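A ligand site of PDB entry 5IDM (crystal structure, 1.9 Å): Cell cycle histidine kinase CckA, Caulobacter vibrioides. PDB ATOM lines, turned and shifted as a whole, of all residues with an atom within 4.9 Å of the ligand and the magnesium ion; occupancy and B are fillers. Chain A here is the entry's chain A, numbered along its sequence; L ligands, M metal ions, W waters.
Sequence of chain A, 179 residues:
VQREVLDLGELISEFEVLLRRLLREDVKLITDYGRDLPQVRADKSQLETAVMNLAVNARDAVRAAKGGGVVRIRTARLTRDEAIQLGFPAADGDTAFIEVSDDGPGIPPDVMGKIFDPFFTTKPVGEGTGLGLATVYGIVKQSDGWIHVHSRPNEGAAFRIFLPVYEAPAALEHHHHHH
Water W7 lies within hydrogen-bond range of O of Asn 53 (2.9 Å) and ND2 of Asn 57 (3.5 Å).
Water W9 lies within hydrogen-bond range of O2 of the ligand, OG1 of Thr 129 and N of Gly 132.
Water W5 lies within hydrogen-bond range of OD1 of Asp 102 (2.7 Å), N5 of the ligand (2.9 Å) and N of Gly 106 (2.9 Å).
Water W6 lies within hydrogen-bond range of ND2 of Asn 57 (2.9 Å) and N3 of the ligand (2.9 Å).
Water W11 bridges O11 of the ligand (3.1 Å) and OG1 of Thr 122 (3.4 Å).
Water W14 lies within hydrogen-bond range of O of Asn 57 (2.8 Å) and N3 of the ligand (3.4 Å).
N of Leu 133 is in hydrogen-bond range of O6 of the ligand (2.8 Å).
An oxygen (O2) of the ligand lies within hydrogen-bond range of the side-chain hydroxyl (OG1) of Thr 129 (3.3 Å).
An oxygen (O2) of the ligand sits at hydrogen-bond distance from the backbone NH of Gly 130, 2.9 Å away.
OD2 of Asp 102 lies within hydrogen-bond range of N4 of the ligand (2.9 Å).
O2 of the ligand lies within hydrogen-bond range of N of Leu 131.
OG1 of Thr 122 is in hydrogen-bond range of O12 of the ligand, at 2.7 Å.
An oxygen (O11) of the ligand is in hydrogen-bond range of the backbone NH of Thr 122, 3.1 Å away.
The side-chain hydroxyl of Thr 121 sits at hydrogen-bond distance from an oxygen (O5) of the ligand.
N of Gly 132 is in hydrogen-bond range of O6 of the ligand (3.4 Å).
N of Thr 129 is in hydrogen-bond range of O2 of the ligand (3.3 Å).
The magnesium ion is bound by O1 of the ligand, at 2.0 Å.
O7 of the ligand binds the magnesium ion (2.1 Å).
O4 of the ligand binds the magnesium ion.
The magnesium ion is bound by OD1 of Asn 57 (2.1 Å).
The magnesium ion is bound by water W10, at 2.1 Å.
Water W7 is bound to the magnesium ion.
The magnesium ion has six donor atoms within binding distance.
The side-chain carboxylate of Asp 60 lies within salt-bridge range of the side-chain amino group of Lys 123, 2.8 Å away.
N of Lys 123 lies within hydrogen-bond range of OG1 of Thr 121, at 3.0 Å.
OG1 of Thr 129 lies within hydrogen-bond range of N of Leu 131 (3.4 Å).
O of Ala 157 is in hydrogen-bond range of N of Asp 102 (2.9 Å).
The backbone carbonyl oxygen (O) of Gly 132 is in hydrogen-bond range of the side-chain amide nitrogen (ND2) of Asn 53, at 3.2 Å.
O of Asn 53 sits close to ND2 of Asn 57.
Ala 61 touches the ligand (CB to N5, 3.5 Å).
Gly 106 touches the ligand (O to C9, 3.8 Å).
CG1 of Ile 107 touches N6 of the ligand (3.6 Å).
CG2 of Ile 115 touches O10 of the ligand (3.8 Å).
Phe 120 touches the ligand (O to C1, 3.4 Å).
Lys 123 touches the ligand (CE to O4, 3.5 Å).
Gly 128 touches the ligand (CA to O3, 3.4 Å).
Ala 157 touches the ligand.
Phe 159 touches the ligand.
Within 4 Å of the ligand: Asn 57, Ala 61, Asp 102, Gly 106, Ile 107, Ile 115, Phe 120, Thr 121, Thr 122, Lys 123, Gly 128, Thr 129, Gly 130, Leu 131, Gly 132, Leu 133, Ala 157 and Phe 159.
Within 4 Å of the magnesium ion: Asn 57.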
ATOM      1  N   ASN A  53      19.079 -32.425  18.644  1.00  0.00           N
ATOM      2  CA  ASN A  53      19.999 -31.307  18.750  1.00  0.00           C
ATOM      3  C   ASN A  53      20.931 -31.452  19.944  1.00  0.00           C
ATOM      4  O   ASN A  53      22.122 -31.179  19.843  1.00  0.00           O
ATOM      5  CB  ASN A  53      19.263 -29.959  18.798  1.00  0.00           C
ATOM      6  CG  ASN A  53      18.646 -29.576  17.461  1.00  0.00           C
ATOM      7  OD1 ASN A  53      18.723 -30.344  16.504  1.00  0.00           O
ATOM      8  ND2 ASN A  53      18.017 -28.402  17.409  1.00  0.00           N
ATOM      9  N   VAL A  56      23.474 -34.497  19.170  1.00  0.00           N
ATOM     10  CA  VAL A  56      24.579 -34.093  18.261  1.00  0.00           C
ATOM     11  C   VAL A  56      25.577 -33.159  18.956  1.00  0.00           C
ATOM     12  O   VAL A  56      26.783 -33.287  18.763  1.00  0.00           O
ATOM     13  CB  VAL A  56      24.140 -33.538  16.871  1.00  0.00           C
ATOM     14  CG1 VAL A  56      23.298 -34.557  16.126  1.00  0.00           C
ATOM     15  CG2 VAL A  56      23.394 -32.219  16.996  1.00  0.00           C
ATOM     16  N   ASN A  57      25.083 -32.252  19.817  1.00  0.00           N
ATOM     17  CA  ASN A  57      25.981 -31.427  20.648  1.00  0.00           C
ATOM     18  C   ASN A  57      26.870 -32.283  21.548  1.00  0.00           C
ATOM     19  O   ASN A  57      28.054 -31.980  21.698  1.00  0.00           O
ATOM     20  CB  ASN A  57      25.193 -30.449  21.528  1.00  0.00           C
ATOM     21  CG  ASN A  57      24.663 -29.249  20.750  1.00  0.00           C
ATOM     22  OD1 ASN A  57      25.080 -29.001  19.625  1.00  0.00           O
ATOM     23  ND2 ASN A  57      23.733 -28.527  21.351  1.00  0.00           N
ATOM     24  N   ALA A  58      26.285 -33.316  22.152  1.00  0.00           N
ATOM     25  CA  ALA A  58      27.048 -34.238  22.990  1.00  0.00           C
ATOM     26  C   ALA A  58      28.121 -34.933  22.161  1.00  0.00           C
ATOM     27  O   ALA A  58      29.284 -35.032  22.585  1.00  0.00           O
ATOM     28  CB  ALA A  58      26.135 -35.243  23.641  1.00  0.00           C
ATOM     29  N   ASP A  60      29.485 -33.820  19.323  1.00  0.00           N
ATOM     30  CA  ASP A  60      30.485 -32.789  19.033  1.00  0.00           C
ATOM     31  C   ASP A  60      31.464 -32.604  20.194  1.00  0.00           C
ATOM     32  O   ASP A  60      32.689 -32.548  20.002  1.00  0.00           O
ATOM     33  CB  ASP A  60      29.811 -31.445  18.725  1.00  0.00           C
ATOM     34  CG  ASP A  60      28.964 -31.466  17.436  1.00  0.00           C
ATOM     35  OD1 ASP A  60      29.021 -32.445  16.673  1.00  0.00           O
ATOM     36  OD2 ASP A  60      28.225 -30.479  17.216  1.00  0.00           O
ATOM     37  N   ALA A  61      30.915 -32.500  21.410  1.00  0.00           N
ATOM     38  CA  ALA A  61      31.688 -32.259  22.614  1.00  0.00           C
ATOM     39  C   ALA A  61      32.719 -33.374  22.895  1.00  0.00           C
ATOM     40  O   ALA A  61      33.838 -33.066  23.297  1.00  0.00           O
ATOM     41  CB  ALA A  61      30.761 -32.078  23.803  1.00  0.00           C
ATOM     42  N   ASP A 102      26.766 -36.075  28.721  1.00  0.00           N
ATOM     43  CA  ASP A 102      28.023 -36.568  28.162  1.00  0.00           C
ATOM     44  C   ASP A 102      29.176 -36.430  29.133  1.00  0.00           C
ATOM     45  O   ASP A 102      29.075 -35.752  30.146  1.00  0.00           O
ATOM     46  CB  ASP A 102      28.342 -35.878  26.829  1.00  0.00           C
ATOM     47  CG  ASP A 102      28.640 -34.389  26.979  1.00  0.00           C
ATOM     48  OD1 ASP A 102      29.692 -34.053  27.583  1.00  0.00           O
ATOM     49  OD2 ASP A 102      27.828 -33.558  26.528  1.00  0.00           O
ATOM     50  N   GLY A 106      32.746 -30.285  29.134  1.00  0.00           N
ATOM     51  CA  GLY A 106      31.849 -29.416  29.874  1.00  0.00           C
ATOM     52  C   GLY A 106      31.844 -28.003  29.317  1.00  0.00           C
ATOM     53  O   GLY A 106      32.554 -27.691  28.363  1.00  0.00           O
ATOM     54  N   ILE A 107      31.025 -27.158  29.919  1.00  0.00           N
ATOM     55  CA  ILE A 107      30.763 -25.830  29.410  1.00  0.00           C
ATOM     56  C   ILE A 107      31.503 -24.830  30.287  1.00  0.00           C
ATOM     57  O   ILE A 107      31.235 -24.787  31.485  1.00  0.00           O
ATOM     58  CB  ILE A 107      29.263 -25.547  29.400  1.00  0.00           C
ATOM     59  CG1 ILE A 107      28.568 -26.523  28.422  1.00  0.00           C
ATOM     60  CG2 ILE A 107      28.966 -24.099  29.034  1.00  0.00           C
ATOM     61  CD1 ILE A 107      27.081 -26.596  28.567  1.00  0.00           C
ATOM     62  N   ILE A 115      24.775 -19.884  25.956  1.00  0.00           N
ATOM     63  CA  ILE A 115      24.644 -21.061  25.073  1.00  0.00           C
ATOM     64  C   ILE A 115      23.278 -21.162  24.361  1.00  0.00           C
ATOM     65  O   ILE A 115      23.206 -21.729  23.277  1.00  0.00           O
ATOM     66  CB  ILE A 115      24.959 -22.395  25.763  1.00  0.00           C
ATOM     67  CG1 ILE A 115      23.998 -22.673  26.926  1.00  0.00           C
ATOM     68  CG2 ILE A 115      26.425 -22.389  26.195  1.00  0.00           C
ATOM     69  CD1 ILE A 115      24.159 -24.058  27.514  1.00  0.00           C
ATOM     70  N   PHE A 120      24.939 -18.175  18.918  1.00  0.00           N
ATOM     71  CA  PHE A 120      26.151 -18.445  19.703  1.00  0.00           C
ATOM     72  C   PHE A 120      26.730 -19.824  19.369  1.00  0.00           C
ATOM     73  O   PHE A 120      26.022 -20.817  19.399  1.00  0.00           O
ATOM     74  CB  PHE A 120      25.946 -18.343  21.216  1.00  0.00           C
ATOM     75  CG  PHE A 120      27.202 -18.684  21.981  1.00  0.00           C
ATOM     76  CD1 PHE A 120      28.229 -17.767  22.061  1.00  0.00           C
ATOM     77  CD2 PHE A 120      27.397 -19.948  22.503  1.00  0.00           C
ATOM     78  CE1 PHE A 120      29.423 -18.095  22.720  1.00  0.00           C
ATOM     79  CE2 PHE A 120      28.582 -20.287  23.159  1.00  0.00           C
ATOM     80  CZ  PHE A 120      29.591 -19.351  23.263  1.00  0.00           C
ATOM     81  N   THR A 121      28.029 -19.864  19.070  1.00  0.00           N
ATOM     82  CA  THR A 121      28.721 -21.108  18.719  1.00  0.00           C
ATOM     83  C   THR A 121      30.196 -20.979  19.046  1.00  0.00           C
ATOM     84  O   THR A 121      30.732 -19.870  19.042  1.00  0.00           O
ATOM     85  CB  THR A 121      28.532 -21.472  17.227  1.00  0.00           C
ATOM     86  OG1 THR A 121      29.108 -22.760  16.919  1.00  0.00           O
ATOM     87  CG2 THR A 121      29.168 -20.411  16.322  1.00  0.00           C
ATOM     88  N   THR A 122      30.841 -22.094  19.344  1.00  0.00           N
ATOM     89  CA  THR A 122      32.304 -22.163  19.431  1.00  0.00           C
ATOM     90  C   THR A 122      32.913 -22.838  18.193  1.00  0.00           C
ATOM     91  O   THR A 122      34.114 -23.046  18.147  1.00  0.00           O
ATOM     92  CB  THR A 122      32.761 -22.914  20.700  1.00  0.00           C
ATOM     93  OG1 THR A 122      32.138 -24.209  20.725  1.00  0.00           O
ATOM     94  CG2 THR A 122      32.356 -22.161  21.952  1.00  0.00           C
ATOM     95  N   LYS A 123      32.092 -23.172  17.189  1.00  0.00           N
ATOM     96  CA  LYS A 123      32.606 -23.828  15.974  1.00  0.00           C
ATOM     97  C   LYS A 123      33.069 -22.796  14.954  1.00  0.00           C
ATOM     98  O   LYS A 123      32.656 -21.652  15.034  1.00  0.00           O
ATOM     99  CB  LYS A 123      31.552 -24.723  15.363  1.00  0.00           C
ATOM    100  CG  LYS A 123      30.963 -25.718  16.329  1.00  0.00           C
ATOM    101  CD  LYS A 123      30.413 -26.869  15.512  1.00  0.00           C
ATOM    102  CE  LYS A 123      29.173 -27.447  16.129  1.00  0.00           C
ATOM    103  NZ  LYS A 123      28.622 -28.529  15.266  1.00  0.00           N
ATOM    104  N   GLU A 127      30.799 -24.241   9.807  1.00  0.00           N
ATOM    105  CA  GLU A 127      30.143 -25.408  10.393  1.00  0.00           C
ATOM    106  C   GLU A 127      28.928 -24.992  11.234  1.00  0.00           C
ATOM    107  O   GLU A 127      29.106 -24.383  12.278  1.00  0.00           O
ATOM    108  CB  GLU A 127      31.105 -26.131  11.349  1.00  0.00           C
ATOM    109  CG  GLU A 127      32.332 -26.809  10.756  1.00  0.00           C
ATOM    110  CD  GLU A 127      33.284 -27.350  11.818  1.00  0.00           C
ATOM    111  OE1 GLU A 127      32.844 -27.602  12.965  1.00  0.00           O
ATOM    112  OE2 GLU A 127      34.486 -27.540  11.505  1.00  0.00           O
ATOM    113  N   GLY A 128      27.723 -25.365  10.819  1.00  0.00           N
ATOM    114  CA  GLY A 128      26.495 -25.084  11.557  1.00  0.00           C
ATOM    115  C   GLY A 128      26.091 -23.627  11.575  1.00  0.00           C
ATOM    116  O   GLY A 128      26.712 -22.797  10.928  1.00  0.00           O
ATOM    117  N   THR A 129      25.028 -23.349  12.318  1.00  0.00           N
ATOM    118  CA  THR A 129      24.447 -22.002  12.403  1.00  0.00           C
ATOM    119  C   THR A 129      24.487 -21.397  13.797  1.00  0.00           C
ATOM    120  O   THR A 129      24.464 -20.168  13.932  1.00  0.00           O
ATOM    121  CB  THR A 129      23.000 -22.023  11.923  1.00  0.00           C
ATOM    122  OG1 THR A 129      22.225 -22.906  12.747  1.00  0.00           O
ATOM    123  CG2 THR A 129      22.927 -22.498  10.466  1.00  0.00           C
ATOM    124  N   GLY A 130      24.590 -22.239  14.828  1.00  0.00           N
ATOM    125  CA  GLY A 130      24.505 -21.769  16.204  1.00  0.00           C
ATOM    126  C   GLY A 130      23.079 -21.592  16.707  1.00  0.00           C
ATOM    127  O   GLY A 130      22.857 -20.881  17.674  1.00  0.00           O
ATOM    128  N   LEU A 131      22.108 -22.219  16.029  1.00  0.00           N
ATOM    129  CA  LEU A 131      20.725 -22.191  16.483  1.00  0.00           C
ATOM    130  C   LEU A 131      20.265 -23.436  17.232  1.00  0.00           C
ATOM    131  O   LEU A 131      19.189 -23.404  17.821  1.00  0.00           O
ATOM    132  CB  LEU A 131      19.764 -21.941  15.313  1.00  0.00           C
ATOM    133  CG  LEU A 131      19.879 -20.575  14.632  1.00  0.00           C
ATOM    134  CD1 LEU A 131      18.995 -20.539  13.403  1.00  0.00           C
ATOM    135  CD2 LEU A 131      19.496 -19.439  15.571  1.00  0.00           C
ATOM    136  N   GLY A 132      21.060 -24.515  17.236  1.00  0.00           N
ATOM    137  CA  GLY A 132      20.664 -25.769  17.878  1.00  0.00           C
ATOM    138  C   GLY A 132      20.010 -25.610  19.241  1.00  0.00           C
ATOM    139  O   GLY A 132      18.888 -26.094  19.450  1.00  0.00           O
ATOM    140  N   LEU A 133      20.673 -24.905  20.151  1.00  0.00           N
ATOM    141  CA  LEU A 133      20.154 -24.759  21.515  1.00  0.00           C
ATOM    142  C   LEU A 133      19.047 -23.713  21.624  1.00  0.00           C
ATOM    143  O   LEU A 133      18.177 -23.824  22.484  1.00  0.00           O
ATOM    144  CB  LEU A 133      21.277 -24.483  22.532  1.00  0.00           C
ATOM    145  CG  LEU A 133      22.101 -25.716  22.945  1.00  0.00           C
ATOM    146  CD1 LEU A 133      23.236 -25.327  23.889  1.00  0.00           C
ATOM    147  CD2 LEU A 133      21.230 -26.765  23.622  1.00  0.00           C
ATOM    148  N   ALA A 134      19.057 -22.689  20.770  1.00  0.00           N
ATOM    149  CA  ALA A 134      17.929 -21.746  20.712  1.00  0.00           C
ATOM    150  C   ALA A 134      16.661 -22.495  20.343  1.00  0.00           C
ATOM    151  O   ALA A 134      15.614 -22.256  20.916  1.00  0.00           O
ATOM    152  CB  ALA A 134      18.200 -20.610  19.718  1.00  0.00           C
ATOM    153  N   ALA A 157      28.645 -32.477  30.556  1.00  0.00           N
ATOM    154  CA  ALA A 157      27.468 -31.611  30.522  1.00  0.00           C
ATOM    155  C   ALA A 157      26.198 -32.443  30.495  1.00  0.00           C
ATOM    156  O   ALA A 157      26.142 -33.468  29.813  1.00  0.00           O
ATOM    157  CB  ALA A 157      27.515 -30.712  29.307  1.00  0.00           C
ATOM    158  N   PHE A 159      22.024 -31.892  30.004  1.00  0.00           N
ATOM    159  CA  PHE A 159      20.928 -31.026  29.607  1.00  0.00           C
ATOM    160  C   PHE A 159      19.664 -31.745  29.991  1.00  0.00           C
ATOM    161  O   PHE A 159      19.383 -32.823  29.469  1.00  0.00           O
ATOM    162  CB  PHE A 159      20.987 -30.762  28.096  1.00  0.00           C
ATOM    163  CG  PHE A 159      22.066 -29.802  27.700  1.00  0.00           C
ATOM    164  CD1 PHE A 159      23.393 -30.199  27.627  1.00  0.00           C
ATOM    165  CD2 PHE A 159      21.755 -28.486  27.381  1.00  0.00           C
ATOM    166  CE1 PHE A 159      24.392 -29.319  27.257  1.00  0.00           C
ATOM    167  CE2 PHE A 159      22.754 -27.590  27.023  1.00  0.00           C
ATOM    168  CZ  PHE A 159      24.075 -28.002  26.955  1.00  0.00           C
HETATM  169  P1  LIG L   1      24.556 -26.073  15.306  1.00  0.00           P
HETATM  170  O1  LIG L   1      23.900 -26.870  16.408  1.00  0.00           O
HETATM  171  O2  LIG L   1      23.659 -24.939  14.861  1.00  0.00           O
HETATM  172  O3  LIG L   1      25.008 -26.833  14.117  1.00  0.00           O
HETATM  173  P2  LIG L   1      26.365 -25.381  17.590  1.00  0.00           P
HETATM  174  O4  LIG L   1      26.313 -26.794  18.044  1.00  0.00           O
HETATM  175  O5  LIG L   1      27.660 -24.639  17.779  1.00  0.00           O
HETATM  176  N1  LIG L   1      26.028 -25.363  15.886  1.00  0.00           N
HETATM  177  P3  LIG L   1      24.270 -25.020  19.522  1.00  0.00           P
HETATM  178  O6  LIG L   1      23.274 -23.944  19.781  1.00  0.00           O
HETATM  179  O7  LIG L   1      23.790 -26.421  19.317  1.00  0.00           O
HETATM  180  O8  LIG L   1      25.165 -24.541  18.282  1.00  0.00           O
HETATM  181  O9  LIG L   1      25.350 -25.016  20.716  1.00  0.00           O
HETATM  182  C1  LIG L   1      25.941 -23.796  21.108  1.00  0.00           C
HETATM  183  C2  LIG L   1      27.281 -24.002  21.803  1.00  0.00           C
HETATM  184  O10 LIG L   1      27.063 -24.455  23.131  1.00  0.00           O
HETATM  185  C3  LIG L   1      28.212 -25.024  21.176  1.00  0.00           C
HETATM  186  O11 LIG L   1      28.958 -24.514  20.064  1.00  0.00           O
HETATM  187  C4  LIG L   1      29.098 -25.355  22.355  1.00  0.00           C
HETATM  188  O12 LIG L   1      30.115 -24.372  22.515  1.00  0.00           O
HETATM  189  C5  LIG L   1      28.142 -25.287  23.533  1.00  0.00           C
HETATM  190  N2  LIG L   1      27.620 -26.628  23.847  1.00  0.00           N
HETATM  191  C6  LIG L   1      26.425 -27.143  23.512  1.00  0.00           C
HETATM  192  N3  LIG L   1      26.305 -28.388  23.987  1.00  0.00           N
HETATM  193  C7  LIG L   1      27.443 -28.683  24.633  1.00  0.00           C
HETATM  194  C8  LIG L   1      27.976 -29.844  25.357  1.00  0.00           C
HETATM  195  N4  LIG L   1      27.237 -30.968  25.485  1.00  0.00           N
HETATM  196  N5  LIG L   1      29.222 -29.735  25.885  1.00  0.00           N
HETATM  197  C9  LIG L   1      29.982 -28.633  25.771  1.00  0.00           C
HETATM  198  N6  LIG L   1      29.538 -27.519  25.113  1.00  0.00           N
HETATM  199  C10 LIG L   1      28.312 -27.509  24.539  1.00  0.00           C
HETATM  200 MG    MG M   1      24.519 -27.830  17.989  1.00  0.00          MG
HETATM  201  O   HOH W   1      31.082 -24.929  25.292  1.00  0.00           O
HETATM  202  O   HOH W   2      24.209 -29.657  14.220  1.00  0.00           O
HETATM  203  O   HOH W   3      27.731 -23.562  14.517  1.00  0.00           O
HETATM  204  O   HOH W   4      23.420 -21.231  20.503  1.00  0.00           O
HETATM  205  O   HOH W   5      30.680 -31.585  27.515  1.00  0.00           O
HETATM  206  O   HOH W   6      23.559 -29.371  24.112  1.00  0.00           O
HETATM  207  O   HOH W   7      22.656 -28.901  18.053  1.00  0.00           O
HETATM  208  O   HOH W   8      24.218 -31.921  24.788  1.00  0.00           O
HETATM  209  O   HOH W   9      20.970 -25.267  14.218  1.00  0.00           O
HETATM  210  O   HOH W  10      25.438 -29.362  16.835  1.00  0.00           O
HETATM  211  O   HOH W  11      30.634 -27.049  19.481  1.00  0.00           O
HETATM  212  O   HOH W  12      23.214 -26.950  11.886  1.00  0.00           O
HETATM  213  O   HOH W  13      21.657 -29.392  15.645  1.00  0.00           O
HETATM  214  O   HOH W  14      28.659 -29.246  21.754  1.00  0.00           O
HETATM  215  O   HOH W  15      28.283 -28.284  19.152  1.00  0.00           O
